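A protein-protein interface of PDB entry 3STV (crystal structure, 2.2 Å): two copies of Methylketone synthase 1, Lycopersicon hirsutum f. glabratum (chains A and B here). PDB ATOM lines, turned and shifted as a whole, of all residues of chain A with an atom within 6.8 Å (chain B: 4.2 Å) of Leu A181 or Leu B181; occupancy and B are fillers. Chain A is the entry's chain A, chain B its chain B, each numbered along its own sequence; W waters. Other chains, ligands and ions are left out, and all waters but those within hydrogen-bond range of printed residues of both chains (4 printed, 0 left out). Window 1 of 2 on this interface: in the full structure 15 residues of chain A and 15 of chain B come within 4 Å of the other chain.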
ATOM      1  N   PHE A  22      20.872  -7.749  -2.416  1.00  0.00           N
ATOM      2  CA  PHE A  22      21.886  -6.690  -2.409  1.00  0.00           C
ATOM      3  C   PHE A  22      22.706  -6.607  -1.123  1.00  0.00           C
ATOM      4  O   PHE A  22      23.807  -6.055  -1.111  1.00  0.00           O
ATOM      5  CB  PHE A  22      21.252  -5.310  -2.638  1.00  0.00           C
ATOM      6  CG  PHE A  22      20.205  -5.286  -3.707  1.00  0.00           C
ATOM      7  CD1 PHE A  22      20.495  -5.722  -5.000  1.00  0.00           C
ATOM      8  CD2 PHE A  22      18.921  -4.811  -3.419  1.00  0.00           C
ATOM      9  CE1 PHE A  22      19.530  -5.683  -5.993  1.00  0.00           C
ATOM     10  CE2 PHE A  22      17.944  -4.767  -4.405  1.00  0.00           C
ATOM     11  CZ  PHE A  22      18.247  -5.205  -5.700  1.00  0.00           C
ATOM     12  N   HIS A  23      22.190  -7.155  -0.035  1.00  0.00           N
ATOM     13  CA  HIS A  23      22.912  -7.060   1.223  1.00  0.00           C
ATOM     14  C   HIS A  23      23.857  -8.200   1.541  1.00  0.00           C
ATOM     15  O   HIS A  23      24.275  -8.945   0.661  1.00  0.00           O
ATOM     16  CB  HIS A  23      21.910  -6.841   2.360  1.00  0.00           C
ATOM     17  CG  HIS A  23      21.261  -5.493   2.313  1.00  0.00           C
ATOM     18  ND1 HIS A  23      20.547  -5.052   1.218  1.00  0.00           N
ATOM     19  CD2 HIS A  23      21.289  -4.456   3.185  1.00  0.00           C
ATOM     20  CE1 HIS A  23      20.169  -3.801   1.416  1.00  0.00           C
ATOM     21  NE2 HIS A  23      20.609  -3.416   2.602  1.00  0.00           N
ATOM     22  N   GLY A  24      24.212  -8.305   2.810  1.00  0.00           N
ATOM     23  CA  GLY A  24      25.117  -9.343   3.248  1.00  0.00           C
ATOM     24  C   GLY A  24      25.057  -9.443   4.751  1.00  0.00           C
ATOM     25  O   GLY A  24      24.271  -8.743   5.398  1.00  0.00           O
ATOM     26  N   ALA A  25      25.876 -10.323   5.309  1.00  0.00           N
ATOM     27  CA  ALA A  25      25.934 -10.521   6.751  1.00  0.00           C
ATOM     28  C   ALA A  25      26.159  -9.191   7.502  1.00  0.00           C
ATOM     29  O   ALA A  25      25.707  -9.021   8.640  1.00  0.00           O
ATOM     30  CB  ALA A  25      27.050 -11.514   7.084  1.00  0.00           C
ATOM     31  N   TRP A  26      26.852  -8.258   6.852  1.00  0.00           N
ATOM     32  CA  TRP A  26      27.163  -6.951   7.439  1.00  0.00           C
ATOM     33  C   TRP A  26      25.953  -6.125   7.879  1.00  0.00           C
ATOM     34  O   TRP A  26      26.031  -5.368   8.838  1.00  0.00           O
ATOM     35  CB  TRP A  26      27.984  -6.104   6.457  1.00  0.00           C
ATOM     36  CG  TRP A  26      27.307  -5.873   5.125  1.00  0.00           C
ATOM     37  CD1 TRP A  26      27.467  -6.614   3.987  1.00  0.00           C
ATOM     38  CD2 TRP A  26      26.345  -4.851   4.805  1.00  0.00           C
ATOM     39  NE1 TRP A  26      26.668  -6.119   2.981  1.00  0.00           N
ATOM     40  CE2 TRP A  26      25.969  -5.039   3.456  1.00  0.00           C
ATOM     41  CE3 TRP A  26      25.767  -3.798   5.529  1.00  0.00           C
ATOM     42  CZ2 TRP A  26      25.035  -4.211   2.812  1.00  0.00           C
ATOM     43  CZ3 TRP A  26      24.837  -2.972   4.891  1.00  0.00           C
ATOM     44  CH2 TRP A  26      24.482  -3.187   3.543  1.00  0.00           C
ATOM     45  N   CYS A  27      24.832  -6.263   7.185  1.00  0.00           N
ATOM     46  CA  CYS A  27      23.656  -5.469   7.535  1.00  0.00           C
ATOM     47  C   CYS A  27      23.103  -5.767   8.931  1.00  0.00           C
ATOM     48  O   CYS A  27      22.386  -4.950   9.502  1.00  0.00           O
ATOM     49  CB  CYS A  27      22.557  -5.668   6.491  1.00  0.00           C
ATOM     50  SG  CYS A  27      21.640  -7.212   6.647  1.00  0.00           S
ATOM     51  N   ASP A  46      26.690 -14.773   4.486  1.00  0.00           N
ATOM     52  CA  ASP A  46      26.662 -13.979   3.267  1.00  0.00           C
ATOM     53  C   ASP A  46      26.177 -15.020   2.274  1.00  0.00           C
ATOM     54  O   ASP A  46      26.729 -16.119   2.228  1.00  0.00           O
ATOM     55  CB  ASP A  46      28.054 -13.536   2.812  1.00  0.00           C
ATOM     56  CG  ASP A  46      28.516 -12.246   3.457  1.00  0.00           C
ATOM     57  OD1 ASP A  46      27.690 -11.335   3.663  1.00  0.00           O
ATOM     58  OD2 ASP A  46      29.729 -12.135   3.732  1.00  0.00           O
ATOM     59  N   SER A  50      27.267 -12.082  -2.128  1.00  0.00           N
ATOM     60  CA  SER A  50      26.770 -11.113  -1.154  1.00  0.00           C
ATOM     61  C   SER A  50      27.864 -10.787  -0.145  1.00  0.00           C
ATOM     62  O   SER A  50      28.671 -11.649   0.197  1.00  0.00           O
ATOM     63  CB  SER A  50      25.539 -11.662  -0.420  1.00  0.00           C
ATOM     64  OG  SER A  50      24.492 -11.931  -1.335  1.00  0.00           O
ATOM     65  N   GLY A  51      27.893  -9.541   0.321  1.00  0.00           N
ATOM     66  CA  GLY A  51      28.906  -9.152   1.276  1.00  0.00           C
ATOM     67  C   GLY A  51      30.276  -9.542   0.759  1.00  0.00           C
ATOM     68  O   GLY A  51      30.662  -9.123  -0.329  1.00  0.00           O
ATOM     69  N   ILE A  52      31.010 -10.347   1.522  1.00  0.00           N
ATOM     70  CA  ILE A  52      32.327 -10.767   1.081  1.00  0.00           C
ATOM     71  C   ILE A  52      32.390 -12.189   0.525  1.00  0.00           C
ATOM     72  O   ILE A  52      33.468 -12.785   0.443  1.00  0.00           O
ATOM     73  CB  ILE A  52      33.378 -10.607   2.197  1.00  0.00           C
ATOM     74  CG1 ILE A  52      32.917 -11.310   3.474  1.00  0.00           C
ATOM     75  CG2 ILE A  52      33.626  -9.130   2.452  1.00  0.00           C
ATOM     76  CD1 ILE A  52      33.977 -11.317   4.571  1.00  0.00           C
ATOM     77  N   ALA A 176      25.121   5.284   4.234  1.00  0.00           N
ATOM     78  CA  ALA A 176      26.486   5.389   3.708  1.00  0.00           C
ATOM     79  C   ALA A 176      27.205   4.033   3.740  1.00  0.00           C
ATOM     80  O   ALA A 176      27.984   3.709   2.846  1.00  0.00           O
ATOM     81  CB  ALA A 176      27.278   6.421   4.519  1.00  0.00           C
ATOM     82  N   LEU A 177      26.945   3.251   4.780  1.00  0.00           N
ATOM     83  CA  LEU A 177      27.546   1.931   4.911  1.00  0.00           C
ATOM     84  C   LEU A 177      27.038   1.042   3.776  1.00  0.00           C
ATOM     85  O   LEU A 177      27.808   0.378   3.071  1.00  0.00           O
ATOM     86  CB  LEU A 177      27.144   1.316   6.251  1.00  0.00           C
ATOM     87  CG  LEU A 177      27.685  -0.071   6.604  1.00  0.00           C
ATOM     88  CD1 LEU A 177      29.206  -0.011   6.684  1.00  0.00           C
ATOM     89  CD2 LEU A 177      27.097  -0.532   7.947  1.00  0.00           C
ATOM     90  N   ALA A 178      25.720   1.049   3.611  1.00  0.00           N
ATOM     91  CA  ALA A 178      25.051   0.257   2.596  1.00  0.00           C
ATOM     92  C   ALA A 178      25.435   0.681   1.179  1.00  0.00           C
ATOM     93  O   ALA A 178      25.589  -0.161   0.293  1.00  0.00           O
ATOM     94  CB  ALA A 178      23.554   0.356   2.788  1.00  0.00           C
ATOM     95  N   THR A 179      25.589   1.985   0.968  1.00  0.00           N
ATOM     96  CA  THR A 179      25.963   2.498  -0.344  1.00  0.00           C
ATOM     97  C   THR A 179      27.325   1.930  -0.768  1.00  0.00           C
ATOM     98  O   THR A 179      27.572   1.706  -1.950  1.00  0.00           O
ATOM     99  CB  THR A 179      26.020   4.054  -0.333  1.00  0.00           C
ATOM    100  OG1 THR A 179      24.700   4.580  -0.155  1.00  0.00           O
ATOM    101  CG2 THR A 179      26.604   4.592  -1.633  1.00  0.00           C
ATOM    102  N   ALA A 180      28.196   1.683   0.206  1.00  0.00           N
ATOM    103  CA  ALA A 180      29.524   1.149  -0.071  1.00  0.00           C
ATOM    104  C   ALA A 180      29.589  -0.377  -0.081  1.00  0.00           C
ATOM    105  O   ALA A 180      30.639  -0.942  -0.391  1.00  0.00           O
ATOM    106  CB  ALA A 180      30.515   1.678   0.954  1.00  0.00           C
ATOM    107  N   LEU A 181      28.481  -1.044   0.237  1.00  0.00           N
ATOM    108  CA  LEU A 181      28.496  -2.506   0.297  1.00  0.00           C
ATOM    109  C   LEU A 181      27.499  -3.293  -0.550  1.00  0.00           C
ATOM    110  O   LEU A 181      27.736  -4.472  -0.841  1.00  0.00           O
ATOM    111  CB  LEU A 181      28.364  -2.955   1.759  1.00  0.00           C
ATOM    112  CG  LEU A 181      29.522  -2.575   2.682  1.00  0.00           C
ATOM    113  CD1 LEU A 181      29.152  -2.879   4.141  1.00  0.00           C
ATOM    114  CD2 LEU A 181      30.769  -3.344   2.259  1.00  0.00           C
ATOM    115  N   VAL A 182      26.382  -2.675  -0.932  1.00  0.00           N
ATOM    116  CA  VAL A 182      25.397  -3.392  -1.733  1.00  0.00           C
ATOM    117  C   VAL A 182      26.015  -3.941  -3.029  1.00  0.00           C
ATOM    118  O   VAL A 182      26.818  -3.279  -3.697  1.00  0.00           O
ATOM    119  CB  VAL A 182      24.170  -2.501  -2.064  1.00  0.00           C
ATOM    120  CG1 VAL A 182      23.408  -2.178  -0.791  1.00  0.00           C
ATOM    121  CG2 VAL A 182      24.612  -1.229  -2.770  1.00  0.00           C
ATOM    122  N   ARG A 183      25.638  -5.164  -3.369  1.00  0.00           N
ATOM    123  CA  ARG A 183      26.160  -5.830  -4.557  1.00  0.00           C
ATOM    124  C   ARG A 183      24.996  -6.275  -5.461  1.00  0.00           C
ATOM    125  O   ARG A 183      23.877  -6.488  -4.988  1.00  0.00           O
ATOM    126  CB  ARG A 183      27.021  -7.037  -4.132  1.00  0.00           C
ATOM    127  CG  ARG A 183      28.282  -6.680  -3.311  1.00  0.00           C
ATOM    128  CD  ARG A 183      29.127  -7.924  -2.949  1.00  0.00           C
ATOM    129  NE  ARG A 183      29.560  -8.649  -4.145  1.00  0.00           N
ATOM    130  CZ  ARG A 183      30.138  -9.851  -4.149  1.00  0.00           C
ATOM    131  NH1 ARG A 183      30.373 -10.497  -3.008  1.00  0.00           N
ATOM    132  NH2 ARG A 183      30.471 -10.421  -5.306  1.00  0.00           N
ATOM    133  N   PRO A 184      25.245  -6.413  -6.775  1.00  0.00           N
ATOM    134  CA  PRO A 184      24.199  -6.826  -7.716  1.00  0.00           C
ATOM    135  C   PRO A 184      23.528  -8.149  -7.380  1.00  0.00           C
ATOM    136  O   PRO A 184      24.136  -9.044  -6.793  1.00  0.00           O
ATOM    137  CB  PRO A 184      24.937  -6.903  -9.054  1.00  0.00           C
ATOM    138  CG  PRO A 184      26.049  -5.910  -8.897  1.00  0.00           C
ATOM    139  CD  PRO A 184      26.516  -6.172  -7.481  1.00  0.00           C
ATOM    140  N   TRP B  26      34.096   0.644   3.304  1.00  0.00           N
ATOM    141  CA  TRP B  26      33.070   0.501   4.333  1.00  0.00           C
ATOM    142  C   TRP B  26      33.440   0.989   5.736  1.00  0.00           C
ATOM    143  O   TRP B  26      32.571   1.449   6.483  1.00  0.00           O
ATOM    144  CB  TRP B  26      32.610  -0.963   4.424  1.00  0.00           C
ATOM    145  CG  TRP B  26      33.700  -1.943   4.759  1.00  0.00           C
ATOM    146  CD1 TRP B  26      34.441  -2.684   3.880  1.00  0.00           C
ATOM    147  CD2 TRP B  26      34.210  -2.250   6.066  1.00  0.00           C
ATOM    148  NE1 TRP B  26      35.382  -3.430   4.555  1.00  0.00           N
ATOM    149  CE2 TRP B  26      35.263  -3.180   5.899  1.00  0.00           C
ATOM    150  CE3 TRP B  26      33.881  -1.826   7.363  1.00  0.00           C
ATOM    151  CZ2 TRP B  26      35.994  -3.693   6.981  1.00  0.00           C
ATOM    152  CZ3 TRP B  26      34.607  -2.336   8.442  1.00  0.00           C
ATOM    153  CH2 TRP B  26      35.652  -3.259   8.241  1.00  0.00           C
ATOM    154  N   ILE B  52      34.218  -4.689  -1.328  1.00  0.00           N
ATOM    155  CA  ILE B  52      33.550  -5.424  -2.395  1.00  0.00           C
ATOM    156  C   ILE B  52      34.278  -5.363  -3.745  1.00  0.00           C
ATOM    157  O   ILE B  52      33.661  -5.513  -4.801  1.00  0.00           O
ATOM    158  CB  ILE B  52      32.079  -4.965  -2.588  1.00  0.00           C
ATOM    159  CG1 ILE B  52      32.024  -3.550  -3.157  1.00  0.00           C
ATOM    160  CG2 ILE B  52      31.330  -5.047  -1.253  1.00  0.00           C
ATOM    161  CD1 ILE B  52      30.616  -3.113  -3.528  1.00  0.00           C
ATOM    162  N   LEU B 177      30.753  -5.510  12.841  1.00  0.00           N
ATOM    163  CA  LEU B 177      30.717  -5.158  11.426  1.00  0.00           C
ATOM    164  C   LEU B 177      32.018  -5.614  10.754  1.00  0.00           C
ATOM    165  O   LEU B 177      32.004  -6.209   9.666  1.00  0.00           O
ATOM    166  CB  LEU B 177      30.543  -3.637  11.265  1.00  0.00           C
ATOM    167  CG  LEU B 177      30.525  -3.082   9.832  1.00  0.00           C
ATOM    168  CD1 LEU B 177      29.315  -3.642   9.099  1.00  0.00           C
ATOM    169  CD2 LEU B 177      30.482  -1.541   9.837  1.00  0.00           C
ATOM    170  N   ALA B 178      33.136  -5.344  11.420  1.00  0.00           N
ATOM    171  CA  ALA B 178      34.462  -5.705  10.913  1.00  0.00           C
ATOM    172  C   ALA B 178      34.689  -7.211  10.784  1.00  0.00           C
ATOM    173  O   ALA B 178      35.301  -7.674   9.816  1.00  0.00           O
ATOM    174  CB  ALA B 178      35.541  -5.095  11.805  1.00  0.00           C
ATOM    175  N   THR B 179      34.205  -7.983  11.749  1.00  0.00           N
ATOM    176  CA  THR B 179      34.392  -9.425  11.680  1.00  0.00           C
ATOM    177  C   THR B 179      33.566 -10.025  10.543  1.00  0.00           C
ATOM    178  O   THR B 179      33.772 -11.171  10.146  1.00  0.00           O
ATOM    179  CB  THR B 179      34.019 -10.112  13.017  1.00  0.00           C
ATOM    180  OG1 THR B 179      32.619  -9.961  13.272  1.00  0.00           O
ATOM    181  CG2 THR B 179      34.803  -9.495  14.160  1.00  0.00           C
ATOM    182  N   ALA B 180      32.630  -9.245  10.013  1.00  0.00           N
ATOM    183  CA  ALA B 180      31.797  -9.713   8.913  1.00  0.00           C
ATOM    184  C   ALA B 180      32.323  -9.214   7.568  1.00  0.00           C
ATOM    185  O   ALA B 180      31.913  -9.709   6.520  1.00  0.00           O
ATOM    186  CB  ALA B 180      30.361  -9.243   9.107  1.00  0.00           C
ATOM    187  N   LEU B 181      33.241  -8.250   7.605  1.00  0.00           N
ATOM    188  CA  LEU B 181      33.769  -7.668   6.376  1.00  0.00           C
ATOM    189  C   LEU B 181      35.272  -7.770   6.093  1.00  0.00           C
ATOM    190  O   LEU B 181      35.675  -7.674   4.931  1.00  0.00           O
ATOM    191  CB  LEU B 181      33.345  -6.198   6.299  1.00  0.00           C
ATOM    192  CG  LEU B 181      31.843  -5.954   6.148  1.00  0.00           C
ATOM    193  CD1 LEU B 181      31.513  -4.473   6.343  1.00  0.00           C
ATOM    194  CD2 LEU B 181      31.403  -6.423   4.774  1.00  0.00           C
ATOM    195  N   VAL B 182      36.104  -7.951   7.118  1.00  0.00           N
ATOM    196  CA  VAL B 182      37.553  -8.029   6.877  1.00  0.00           C
ATOM    197  C   VAL B 182      37.923  -9.151   5.922  1.00  0.00           C
ATOM    198  O   VAL B 182      37.379 -10.252   5.992  1.00  0.00           O
ATOM    199  CB  VAL B 182      38.372  -8.215   8.183  1.00  0.00           C
ATOM    200  CG1 VAL B 182      38.296  -6.944   9.022  1.00  0.00           C
ATOM    201  CG2 VAL B 182      37.867  -9.423   8.966  1.00  0.00           C
ATOM    202  N   ARG B 183      38.863  -8.866   5.031  1.00  0.00           N
ATOM    203  CA  ARG B 183      39.294  -9.851   4.050  1.00  0.00           C
ATOM    204  C   ARG B 183      40.798 -10.116   4.131  1.00  0.00           C
ATOM    205  O   ARG B 183      41.567  -9.288   4.638  1.00  0.00           O
ATOM    206  CB  ARG B 183      38.911  -9.381   2.635  1.00  0.00           C
ATOM    207  CG  ARG B 183      37.400  -9.324   2.385  1.00  0.00           C
ATOM    208  CD  ARG B 183      37.053  -8.790   1.000  1.00  0.00           C
ATOM    209  NE  ARG B 183      37.549  -9.652  -0.077  1.00  0.00           N
ATOM    210  CZ  ARG B 183      37.561  -9.314  -1.365  1.00  0.00           C
ATOM    211  NH1 ARG B 183      37.103  -8.127  -1.753  1.00  0.00           N
ATOM    212  NH2 ARG B 183      38.044 -10.161  -2.267  1.00  0.00           N
HETATM  213  O   HOH W   1      36.041 -12.710  -1.110  1.00  0.00           O
HETATM  214  O   HOH W   2      33.575  -1.335   1.076  1.00  0.00           O
HETATM  215  O   HOH W   3      30.985 -12.326   5.900  1.00  0.00           O
HETATM  216  O   HOH W   4      28.865  -9.331   5.195  1.00  0.00           O
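Water W3 lies within hydrogen-bond range of OD2 of Asp A46 and O of Ala B180.
Water W4 lies within hydrogen-bond range of the side-chain carboxylate of Asp A46 (2.8 Å), the backbone NH of Trp A26 (2.8 Å), the backbone NH of Ala A25 (3.2 Å) and the backbone carbonyl oxygen of Ala B180 (3.3 Å).
Water W1 lies within hydrogen-bond range of O of Ile A52 (3.0 Å) and NH2 of Arg B183 (3.4 Å).
Water W2 bridges N of Trp B26 (3.0 Å) and O of Ala A180 (3.3 Å).
Among the printed residues, merely in contact across the chains: Trp A26 with Leu B177 (3.7 Å), Trp A26 with Leu B181 (3.8 Å), Ile A52 with Ala B180 (3.3 Å), Ile A52 with Leu B181 (3.5 Å), Ile A52 with Val B182 (3.8 Å), Ile A52 with Arg B183 (3.7 Å), Leu A177 with Trp B26 (3.7 Å), Leu A177 with Leu B177 (3.7 Å), Ala A180 with Ile B52 (3.8 Å), Leu A181 with Trp B26 (3.7 Å), Leu A181 with Ile B52 (3.7 Å), Leu A181 with Leu B181 (3.6 Å) and Val A182 with Ile B52 (3.8 Å).
Ile A52 touches Ala B180, and with the chains exchanged Ala A180 touches Ile B52.
Ile A52 touches Leu B181, and with the chains exchanged Leu A181 touches Ile B52.
Ile A52 touches Arg B183, but with the chains exchanged Arg A183 does not touch Ile B52 (4.001 Å).
Leu B177 touches its own counterpart, Leu A177.
9 positions are printed for both chains.
Of the 13 pairs that touch across the chains among the printed residues, 12 have their exchanged pair printed and touching as well.
The backbone NH of Ile A52 lies within hydrogen-bond range of the side-chain carboxylate of Asp A46.
Of the printed residues of chain B, Ile A52 touches Ala B180, Leu B181, Val B182 and Arg B183.
Ala A178 touches none of the printed residues of chain B.
Of the printed residues of chain B, Ala A180 touches Ile B52.
Leu A181 touches three residues of chain B.
Of the printed residues of chain A, Trp B26 touches Leu A177 and Leu A181.
Of the printed residues of chain A, Ile B52 touches Ala A180, Leu A181 and Val A182.
Printed residues of chain A within 4 Å of Leu B177: Trp A26 (3.7 Å) and Leu A177 (3.7 Å).
Thr B179 touches none of the printed residues of chain A.
Of the printed residues of chain A, Leu B181 touches Trp A26 (3.8 Å), Ile A52 (3.5 Å) and Leu A181 (3.6 Å).
The nearest printed residue of chain B that does not touch Leu A181 is Leu B177 (5.0 Å).
The nearest residue of chain A that does not touch Leu B181 is Leu A177 (5.0 Å).
The nearest printed residue of chain A that does not touch Arg B183 is Gly A51 (6.5 Å).
Hydrophobic or aromatic side chains of chain A that line the printed part of chain B: Trp A26, Ile A52, Leu A177 and Leu A181.
Printed residues of chain B that touch a printed residue of chain A: Trp B26, Ile B52, Leu B177, Ala B180, Leu B181, Val B182 and Arg B183.
Hydrophobic or aromatic side chains of chain B that line the printed part of chain A: Trp B26, Ile B52, Leu B177 and Leu B181.
Among the printed residues, 13 pairs touch across the chains.
Among the printed residues, no Asp or Glu carboxylate lies within 4 Å of a Lys or Arg side-chain nitrogen of the other chain.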
